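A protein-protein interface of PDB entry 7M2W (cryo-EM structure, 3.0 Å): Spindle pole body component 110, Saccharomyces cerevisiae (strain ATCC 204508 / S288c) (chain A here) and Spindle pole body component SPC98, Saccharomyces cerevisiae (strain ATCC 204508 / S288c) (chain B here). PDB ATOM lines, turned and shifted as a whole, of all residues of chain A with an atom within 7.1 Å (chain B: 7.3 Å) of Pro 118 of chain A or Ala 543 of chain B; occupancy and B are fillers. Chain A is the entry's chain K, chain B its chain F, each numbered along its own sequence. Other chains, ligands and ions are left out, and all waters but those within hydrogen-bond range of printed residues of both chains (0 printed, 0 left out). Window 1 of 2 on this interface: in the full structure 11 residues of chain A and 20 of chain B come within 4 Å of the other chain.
Hydrophobic or aromatic side chains of chain A that line the printed part of chain B: Pro 118 and Leu 119.
Among the printed residues, 18 pairs touch across the chains.
Among the printed residues, no Asp or Glu carboxylate lies within 4 Å of a Lys or Arg side-chain nitrogen of the other chain.
The side-chain hydroxyl (OG) of Ser 116 of chain A is in hydrogen-bond range of the side-chain amide oxygen (OE1) of Gln 117 of chain A.
OE2 of Glu 121 of chain A lies within salt-bridge range of NE of Arg 125 of chain A.
The backbone carbonyl oxygen of Thr 559 of chain B sits at hydrogen-bond distance from the backbone NH of Arg 544 of chain B (2.9 Å).
The backbone carbonyl oxygen (O) of Gly 540 of chain B is in hydrogen-bond range of the backbone NH (N) of Ile 563 of chain B.
O of Asp 542 of chain B sits at hydrogen-bond distance from N of Asp 561 of chain B, 2.8 Å away.
NH2 of Arg 544 of chain B is in salt-bridge range of OD2 of Asp 561 of chain B, at 3.4 Å.
Pro 118 of chain A touches just these residues of chain B: Asp 542, Ala 543, Arg 544 and Ile 563.
Ala 543 of chain B touches just these residues of chain A: Pro 118 and Leu 119.
Printed residues of chain A within 4 Å of Val 545 of chain B: Ser 116 (2.9 Å) and Leu 119 (3.9 Å).
Of the printed residues of chain A, Leu 541 of chain B touches Lys 120 (3.8 Å).
Of the printed residues of chain B, Gln 117 of chain A touches Arg 544.
The nearest residue of chain B that does not touch Pro 118 of chain A is Asp 561 of chain B (5.6 Å).
O of Ala 543 of chain B is in hydrogen-bond range of N of Leu 119 of chain A, 3.2 Å away.
OD1 of Asp 542 of chain B is in hydrogen-bond range of N of Glu 121 of chain A, at 3.1 Å.
The guanidinium group of Arg 544 of chain B sits at hydrogen-bond distance from the backbone carbonyl oxygen of Ser 116 of chain A.
OH of Tyr 565 of chain B is in hydrogen-bond range of OE1 of Glu 121 of chain A (3.1 Å).
N of Ser 116 of chain A sits at hydrogen-bond distance from O of Val 545 of chain B.
OE2 of Glu 123 of chain A lies close to O of Asn 509 of chain B (3.4 Å).
Among the printed residues, merely in contact across the chains: Gln 117 of chain A with Arg 544 of chain B, Pro 118 of chain A with Asp 542 of chain B, Pro 118 of chain A with Ala 543 of chain B, Pro 118 of chain A with Arg 544 of chain B, Pro 118 of chain A with Ile 563 of chain B, Leu 119 of chain A with Leu 512 of chain B, Leu 119 of chain A with Val 545 of chain B, Lys 120 of chain A with Thr 513 of chain B, Lys 120 of chain A with Leu 541 of chain B, Lys 120 of chain A with Asp 542 of chain B, Glu 121 of chain A with Ile 563 of chain B and Glu 123 of chain A with Thr 513 of chain B.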
ATOM      1  N   SER A 116     -13.929 -16.811  22.726  1.00  0.00           N
ATOM      2  CA  SER A 116     -13.979 -17.195  24.124  1.00  0.00           C
ATOM      3  C   SER A 116     -14.287 -15.988  25.004  1.00  0.00           C
ATOM      4  O   SER A 116     -14.185 -14.831  24.588  1.00  0.00           O
ATOM      5  CB  SER A 116     -12.658 -17.834  24.549  1.00  0.00           C
ATOM      6  OG  SER A 116     -12.676 -18.166  25.925  1.00  0.00           O
ATOM      7  N   GLN A 117     -14.666 -16.274  26.246  1.00  0.00           N
ATOM      8  CA  GLN A 117     -14.899 -15.241  27.245  1.00  0.00           C
ATOM      9  C   GLN A 117     -13.575 -14.548  27.546  1.00  0.00           C
ATOM     10  O   GLN A 117     -12.521 -15.040  27.125  1.00  0.00           O
ATOM     11  CB  GLN A 117     -15.512 -15.851  28.511  1.00  0.00           C
ATOM     12  CG  GLN A 117     -14.563 -16.721  29.318  1.00  0.00           C
ATOM     13  CD  GLN A 117     -14.588 -18.173  28.887  1.00  0.00           C
ATOM     14  OE1 GLN A 117     -15.154 -18.513  27.850  1.00  0.00           O
ATOM     15  NE2 GLN A 117     -13.969 -19.038  29.681  1.00  0.00           N
ATOM     16  N   PRO A 118     -13.575 -13.411  28.245  1.00  0.00           N
ATOM     17  CA  PRO A 118     -12.301 -12.771  28.605  1.00  0.00           C
ATOM     18  C   PRO A 118     -11.406 -13.730  29.376  1.00  0.00           C
ATOM     19  O   PRO A 118     -11.877 -14.712  29.949  1.00  0.00           O
ATOM     20  CB  PRO A 118     -12.731 -11.582  29.469  1.00  0.00           C
ATOM     21  CG  PRO A 118     -14.102 -11.278  29.015  1.00  0.00           C
ATOM     22  CD  PRO A 118     -14.729 -12.571  28.608  1.00  0.00           C
ATOM     23  N   LEU A 119     -10.104 -13.442  29.381  1.00  0.00           N
ATOM     24  CA  LEU A 119      -9.159 -14.349  30.023  1.00  0.00           C
ATOM     25  C   LEU A 119      -8.783 -13.864  31.415  1.00  0.00           C
ATOM     26  O   LEU A 119      -8.885 -14.621  32.391  1.00  0.00           O
ATOM     27  CB  LEU A 119      -7.915 -14.510  29.154  1.00  0.00           C
ATOM     28  CG  LEU A 119      -8.166 -15.080  27.758  1.00  0.00           C
ATOM     29  CD1 LEU A 119      -6.879 -15.116  26.963  1.00  0.00           C
ATOM     30  CD2 LEU A 119      -8.783 -16.462  27.847  1.00  0.00           C
ATOM     31  N   LYS A 120      -8.337 -12.613  31.527  1.00  0.00           N
ATOM     32  CA  LYS A 120      -8.041 -12.053  32.842  1.00  0.00           C
ATOM     33  C   LYS A 120      -9.266 -12.107  33.744  1.00  0.00           C
ATOM     34  O   LYS A 120      -9.167 -12.506  34.911  1.00  0.00           O
ATOM     35  CB  LYS A 120      -7.536 -10.617  32.699  1.00  0.00           C
ATOM     36  CG  LYS A 120      -6.834 -10.075  33.932  1.00  0.00           C
ATOM     37  CD  LYS A 120      -6.339  -8.656  33.705  1.00  0.00           C
ATOM     38  CE  LYS A 120      -7.453  -7.643  33.905  1.00  0.00           C
ATOM     39  NZ  LYS A 120      -6.941  -6.245  33.940  1.00  0.00           N
ATOM     40  N   GLU A 121     -10.432 -11.734  33.211  1.00  0.00           N
ATOM     41  CA  GLU A 121     -11.665 -11.818  33.984  1.00  0.00           C
ATOM     42  C   GLU A 121     -11.985 -13.256  34.366  1.00  0.00           C
ATOM     43  O   GLU A 121     -12.411 -13.513  35.495  1.00  0.00           O
ATOM     44  CB  GLU A 121     -12.824 -11.209  33.198  1.00  0.00           C
ATOM     45  CG  GLU A 121     -14.185 -11.428  33.837  1.00  0.00           C
ATOM     46  CD  GLU A 121     -15.330 -11.165  32.880  1.00  0.00           C
ATOM     47  OE1 GLU A 121     -15.167 -10.318  31.978  1.00  0.00           O
ATOM     48  OE2 GLU A 121     -16.391 -11.807  33.029  1.00  0.00           O
ATOM     49  N   GLN A 122     -11.792 -14.199  33.443  1.00  0.00           N
ATOM     50  CA  GLN A 122     -12.057 -15.601  33.750  1.00  0.00           C
ATOM     51  C   GLN A 122     -11.204 -16.088  34.915  1.00  0.00           C
ATOM     52  O   GLN A 122     -11.718 -16.706  35.854  1.00  0.00           O
ATOM     53  CB  GLN A 122     -11.809 -16.459  32.511  1.00  0.00           C
ATOM     54  CG  GLN A 122     -11.755 -17.950  32.778  1.00  0.00           C
ATOM     55  CD  GLN A 122     -13.057 -18.493  33.331  1.00  0.00           C
ATOM     56  OE1 GLN A 122     -14.123 -17.913  33.125  1.00  0.00           O
ATOM     57  NE2 GLN A 122     -12.976 -19.614  34.034  1.00  0.00           N
ATOM     58  N   GLU A 123      -9.901 -15.810  34.881  1.00  0.00           N
ATOM     59  CA  GLU A 123      -9.034 -16.313  35.942  1.00  0.00           C
ATOM     60  C   GLU A 123      -9.289 -15.588  37.258  1.00  0.00           C
ATOM     61  O   GLU A 123      -9.212 -16.199  38.335  1.00  0.00           O
ATOM     62  CB  GLU A 123      -7.571 -16.193  35.528  1.00  0.00           C
ATOM     63  CG  GLU A 123      -7.306 -16.703  34.129  1.00  0.00           C
ATOM     64  CD  GLU A 123      -5.861 -16.548  33.724  1.00  0.00           C
ATOM     65  OE1 GLU A 123      -5.020 -16.310  34.615  1.00  0.00           O
ATOM     66  OE2 GLU A 123      -5.570 -16.642  32.515  1.00  0.00           O
ATOM     67  N   ARG A 125     -12.216 -14.536  38.178  1.00  0.00           N
ATOM     68  CA  ARG A 125     -13.420 -15.193  38.676  1.00  0.00           C
ATOM     69  C   ARG A 125     -13.098 -16.542  39.298  1.00  0.00           C
ATOM     70  O   ARG A 125     -13.684 -16.912  40.316  1.00  0.00           O
ATOM     71  CB  ARG A 125     -14.447 -15.365  37.557  1.00  0.00           C
ATOM     72  CG  ARG A 125     -15.089 -14.081  37.071  1.00  0.00           C
ATOM     73  CD  ARG A 125     -16.112 -14.374  35.984  1.00  0.00           C
ATOM     74  NE  ARG A 125     -15.485 -14.920  34.783  1.00  0.00           N
ATOM     75  CZ  ARG A 125     -16.154 -15.395  33.739  1.00  0.00           C
ATOM     76  NH1 ARG A 125     -17.480 -15.394  33.740  1.00  0.00           N
ATOM     77  NH2 ARG A 125     -15.496 -15.873  32.691  1.00  0.00           N
ATOM     78  N   ASN B 509      -3.376 -20.008  27.345  1.00  0.00           N
ATOM     79  CA  ASN B 509      -4.675 -19.436  27.714  1.00  0.00           C
ATOM     80  C   ASN B 509      -4.680 -18.902  29.145  1.00  0.00           C
ATOM     81  O   ASN B 509      -5.670 -18.327  29.604  1.00  0.00           O
ATOM     82  CB  ASN B 509      -5.816 -20.440  27.516  1.00  0.00           C
ATOM     83  CG  ASN B 509      -6.243 -20.566  26.068  1.00  0.00           C
ATOM     84  OD1 ASN B 509      -7.257 -20.003  25.659  1.00  0.00           O
ATOM     85  ND2 ASN B 509      -5.487 -21.329  25.293  1.00  0.00           N
ATOM     86  N   LEU B 512      -1.378 -15.853  29.058  1.00  0.00           N
ATOM     87  CA  LEU B 512      -1.685 -14.637  28.314  1.00  0.00           C
ATOM     88  C   LEU B 512      -2.009 -13.456  29.214  1.00  0.00           C
ATOM     89  O   LEU B 512      -1.662 -12.325  28.868  1.00  0.00           O
ATOM     90  CB  LEU B 512      -2.848 -14.880  27.351  1.00  0.00           C
ATOM     91  CG  LEU B 512      -2.521 -15.752  26.141  1.00  0.00           C
ATOM     92  CD1 LEU B 512      -3.766 -16.054  25.328  1.00  0.00           C
ATOM     93  CD2 LEU B 512      -1.485 -15.052  25.285  1.00  0.00           C
ATOM     94  N   THR B 513      -2.663 -13.679  30.353  1.00  0.00           N
ATOM     95  CA  THR B 513      -2.917 -12.563  31.256  1.00  0.00           C
ATOM     96  C   THR B 513      -1.627 -12.004  31.845  1.00  0.00           C
ATOM     97  O   THR B 513      -1.476 -10.780  31.943  1.00  0.00           O
ATOM     98  CB  THR B 513      -3.882 -12.987  32.365  1.00  0.00           C
ATOM     99  OG1 THR B 513      -4.170 -11.863  33.206  1.00  0.00           O
ATOM    100  CG2 THR B 513      -3.308 -14.122  33.197  1.00  0.00           C
ATOM    101  N   LEU B 516      -0.016 -10.008  29.202  1.00  0.00           N
ATOM    102  CA  LEU B 516      -0.649  -8.700  29.068  1.00  0.00           C
ATOM    103  C   LEU B 516      -0.177  -7.742  30.152  1.00  0.00           C
ATOM    104  O   LEU B 516       0.144  -6.582  29.868  1.00  0.00           O
ATOM    105  CB  LEU B 516      -2.169  -8.844  29.109  1.00  0.00           C
ATOM    106  CG  LEU B 516      -2.840  -9.297  27.815  1.00  0.00           C
ATOM    107  CD1 LEU B 516      -4.347  -9.318  27.978  1.00  0.00           C
ATOM    108  CD2 LEU B 516      -2.442  -8.387  26.673  1.00  0.00           C
ATOM    109  N   GLY B 540      -9.520  -2.853  32.504  1.00  0.00           N
ATOM    110  CA  GLY B 540     -10.440  -3.415  31.536  1.00  0.00           C
ATOM    111  C   GLY B 540      -9.800  -4.083  30.342  1.00  0.00           C
ATOM    112  O   GLY B 540     -10.521  -4.577  29.471  1.00  0.00           O
ATOM    113  N   LEU B 541      -8.474  -4.119  30.276  1.00  0.00           N
ATOM    114  CA  LEU B 541      -7.796  -4.743  29.149  1.00  0.00           C
ATOM    115  C   LEU B 541      -7.755  -6.254  29.329  1.00  0.00           C
ATOM    116  O   LEU B 541      -7.076  -6.766  30.224  1.00  0.00           O
ATOM    117  CB  LEU B 541      -6.380  -4.191  29.000  1.00  0.00           C
ATOM    118  CG  LEU B 541      -5.454  -5.021  28.112  1.00  0.00           C
ATOM    119  CD1 LEU B 541      -5.967  -5.060  26.686  1.00  0.00           C
ATOM    120  CD2 LEU B 541      -4.050  -4.461  28.153  1.00  0.00           C
ATOM    121  N   ASP B 542      -8.485  -6.965  28.475  1.00  0.00           N
ATOM    122  CA  ASP B 542      -8.543  -8.416  28.522  1.00  0.00           C
ATOM    123  C   ASP B 542      -8.347  -8.953  27.112  1.00  0.00           C
ATOM    124  O   ASP B 542      -8.537  -8.244  26.122  1.00  0.00           O
ATOM    125  CB  ASP B 542      -9.863  -8.905  29.116  1.00  0.00           C
ATOM    126  CG  ASP B 542     -10.095  -8.402  30.525  1.00  0.00           C
ATOM    127  OD1 ASP B 542     -10.164  -9.237  31.450  1.00  0.00           O
ATOM    128  OD2 ASP B 542     -10.219  -7.173  30.709  1.00  0.00           O
ATOM    129  N   ALA B 543      -7.968 -10.225  27.029  1.00  0.00           N
ATOM    130  CA  ALA B 543      -7.737 -10.868  25.747  1.00  0.00           C
ATOM    131  C   ALA B 543      -8.815 -11.912  25.517  1.00  0.00           C
ATOM    132  O   ALA B 543      -9.444 -12.402  26.458  1.00  0.00           O
ATOM    133  CB  ALA B 543      -6.348 -11.507  25.681  1.00  0.00           C
ATOM    134  N   ARG B 544      -9.034 -12.239  24.248  1.00  0.00           N
ATOM    135  CA  ARG B 544      -9.984 -13.270  23.867  1.00  0.00           C
ATOM    136  C   ARG B 544      -9.337 -14.220  22.872  1.00  0.00           C
ATOM    137  O   ARG B 544      -8.496 -13.827  22.059  1.00  0.00           O
ATOM    138  CB  ARG B 544     -11.260 -12.674  23.267  1.00  0.00           C
ATOM    139  CG  ARG B 544     -12.021 -11.764  24.207  1.00  0.00           C
ATOM    140  CD  ARG B 544     -13.254 -11.214  23.530  1.00  0.00           C
ATOM    141  NE  ARG B 544     -14.144 -10.539  24.467  1.00  0.00           N
ATOM    142  CZ  ARG B 544     -15.158 -11.132  25.088  1.00  0.00           C
ATOM    143  NH1 ARG B 544     -15.407 -12.416  24.873  1.00  0.00           N
ATOM    144  NH2 ARG B 544     -15.921 -10.443  25.924  1.00  0.00           N
ATOM    145  N   VAL B 545      -9.744 -15.482  22.948  1.00  0.00           N
ATOM    146  CA  VAL B 545      -9.231 -16.545  22.093  1.00  0.00           C
ATOM    147  C   VAL B 545     -10.319 -16.911  21.094  1.00  0.00           C
ATOM    148  O   VAL B 545     -11.382 -17.410  21.480  1.00  0.00           O
ATOM    149  CB  VAL B 545      -8.796 -17.764  22.918  1.00  0.00           C
ATOM    150  CG1 VAL B 545      -8.267 -18.861  22.017  1.00  0.00           C
ATOM    151  CG2 VAL B 545      -7.746 -17.353  23.932  1.00  0.00           C
ATOM    152  N   PHE B 558      -5.467 -15.208  18.501  1.00  0.00           N
ATOM    153  CA  PHE B 558      -5.380 -14.263  19.604  1.00  0.00           C
ATOM    154  C   PHE B 558      -5.849 -12.884  19.169  1.00  0.00           C
ATOM    155  O   PHE B 558      -5.419 -12.367  18.136  1.00  0.00           O
ATOM    156  CB  PHE B 558      -3.943 -14.182  20.109  1.00  0.00           C
ATOM    157  CG  PHE B 558      -3.744 -13.214  21.237  1.00  0.00           C
ATOM    158  CD1 PHE B 558      -4.059 -13.568  22.534  1.00  0.00           C
ATOM    159  CD2 PHE B 558      -3.240 -11.947  20.998  1.00  0.00           C
ATOM    160  CE1 PHE B 558      -3.869 -12.681  23.572  1.00  0.00           C
ATOM    161  CE2 PHE B 558      -3.052 -11.054  22.031  1.00  0.00           C
ATOM    162  CZ  PHE B 558      -3.367 -11.421  23.320  1.00  0.00           C
ATOM    163  N   THR B 559      -6.735 -12.289  19.964  1.00  0.00           N
ATOM    164  CA  THR B 559      -7.160 -10.914  19.763  1.00  0.00           C
ATOM    165  C   THR B 559      -7.290 -10.235  21.115  1.00  0.00           C
ATOM    166  O   THR B 559      -7.527 -10.879  22.138  1.00  0.00           O
ATOM    167  CB  THR B 559      -8.493 -10.824  19.013  1.00  0.00           C
ATOM    168  OG1 THR B 559      -9.391 -11.822  19.510  1.00  0.00           O
ATOM    169  CG2 THR B 559      -8.283 -11.033  17.531  1.00  0.00           C
ATOM    170  N   LEU B 560      -7.136  -8.918  21.108  1.00  0.00           N
ATOM    171  CA  LEU B 560      -7.335  -8.117  22.303  1.00  0.00           C
ATOM    172  C   LEU B 560      -8.770  -7.623  22.363  1.00  0.00           C
ATOM    173  O   LEU B 560      -9.469  -7.555  21.350  1.00  0.00           O
ATOM    174  CB  LEU B 560      -6.377  -6.927  22.345  1.00  0.00           C
ATOM    175  CG  LEU B 560      -4.905  -7.270  22.538  1.00  0.00           C
ATOM    176  CD1 LEU B 560      -4.059  -6.014  22.498  1.00  0.00           C
ATOM    177  CD2 LEU B 560      -4.715  -8.012  23.842  1.00  0.00           C
ATOM    178  N   ASP B 561      -9.203  -7.279  23.569  1.00  0.00           N
ATOM    179  CA  ASP B 561     -10.538  -6.756  23.793  1.00  0.00           C
ATOM    180  C   ASP B 561     -10.465  -5.712  24.894  1.00  0.00           C
ATOM    181  O   ASP B 561      -9.383  -5.306  25.327  1.00  0.00           O
ATOM    182  CB  ASP B 561     -11.523  -7.874  24.154  1.00  0.00           C
ATOM    183  CG  ASP B 561     -12.955  -7.521  23.807  1.00  0.00           C
ATOM    184  OD1 ASP B 561     -13.162  -6.518  23.092  1.00  0.00           O
ATOM    185  OD2 ASP B 561     -13.873  -8.232  24.262  1.00  0.00           O
ATOM    186  N   TYR B 562     -11.633  -5.278  25.350  1.00  0.00           N
ATOM    187  CA  TYR B 562     -11.729  -4.315  26.434  1.00  0.00           C
ATOM    188  C   TYR B 562     -13.055  -4.555  27.128  1.00  0.00           C
ATOM    189  O   TYR B 562     -14.113  -4.397  26.514  1.00  0.00           O
ATOM    190  CB  TYR B 562     -11.641  -2.882  25.910  1.00  0.00           C
ATOM    191  CG  TYR B 562     -11.229  -1.870  26.947  1.00  0.00           C
ATOM    192  CD1 TYR B 562      -9.891  -1.614  27.197  1.00  0.00           C
ATOM    193  CD2 TYR B 562     -12.176  -1.170  27.674  1.00  0.00           C
ATOM    194  CE1 TYR B 562      -9.509  -0.688  28.141  1.00  0.00           C
ATOM    195  CE2 TYR B 562     -11.803  -0.244  28.619  1.00  0.00           C
ATOM    196  CZ  TYR B 562     -10.471  -0.005  28.849  1.00  0.00           C
ATOM    197  OH  TYR B 562     -10.101   0.919  29.794  1.00  0.00           O
ATOM    198  N   ILE B 563     -12.998  -4.944  28.397  1.00  0.00           N
ATOM    199  CA  ILE B 563     -14.179  -5.357  29.142  1.00  0.00           C
ATOM    200  C   ILE B 563     -14.729  -4.141  29.864  1.00  0.00           C
ATOM    201  O   ILE B 563     -14.198  -3.731  30.903  1.00  0.00           O
ATOM    202  CB  ILE B 563     -13.867  -6.497  30.118  1.00  0.00           C
ATOM    203  CG1 ILE B 563     -13.292  -7.687  29.352  1.00  0.00           C
ATOM    204  CG2 ILE B 563     -15.117  -6.902  30.871  1.00  0.00           C
ATOM    205  CD1 ILE B 563     -13.977  -7.947  28.022  1.00  0.00           C
ATOM    206  N   TYR B 565     -17.753  -2.202  31.858  1.00  0.00           N
ATOM    207  CA  TYR B 565     -18.880  -2.381  32.755  1.00  0.00           C
ATOM    208  C   TYR B 565     -19.555  -1.031  32.917  1.00  0.00           C
ATOM    209  O   TYR B 565     -18.962   0.003  32.592  1.00  0.00           O
ATOM    210  CB  TYR B 565     -18.412  -2.930  34.110  1.00  0.00           C
ATOM    211  CG  TYR B 565     -17.971  -4.372  34.038  1.00  0.00           C
ATOM    212  CD1 TYR B 565     -16.717  -4.759  34.485  1.00  0.00           C
ATOM    213  CD2 TYR B 565     -18.809  -5.344  33.512  1.00  0.00           C
ATOM    214  CE1 TYR B 565     -16.312  -6.078  34.417  1.00  0.00           C
ATOM    215  CE2 TYR B 565     -18.414  -6.662  33.439  1.00  0.00           C
ATOM    216  CZ  TYR B 565     -17.166  -7.024  33.893  1.00  0.00           C
ATOM    217  OH  TYR B 565     -16.769  -8.339  33.822  1.00  0.00           O
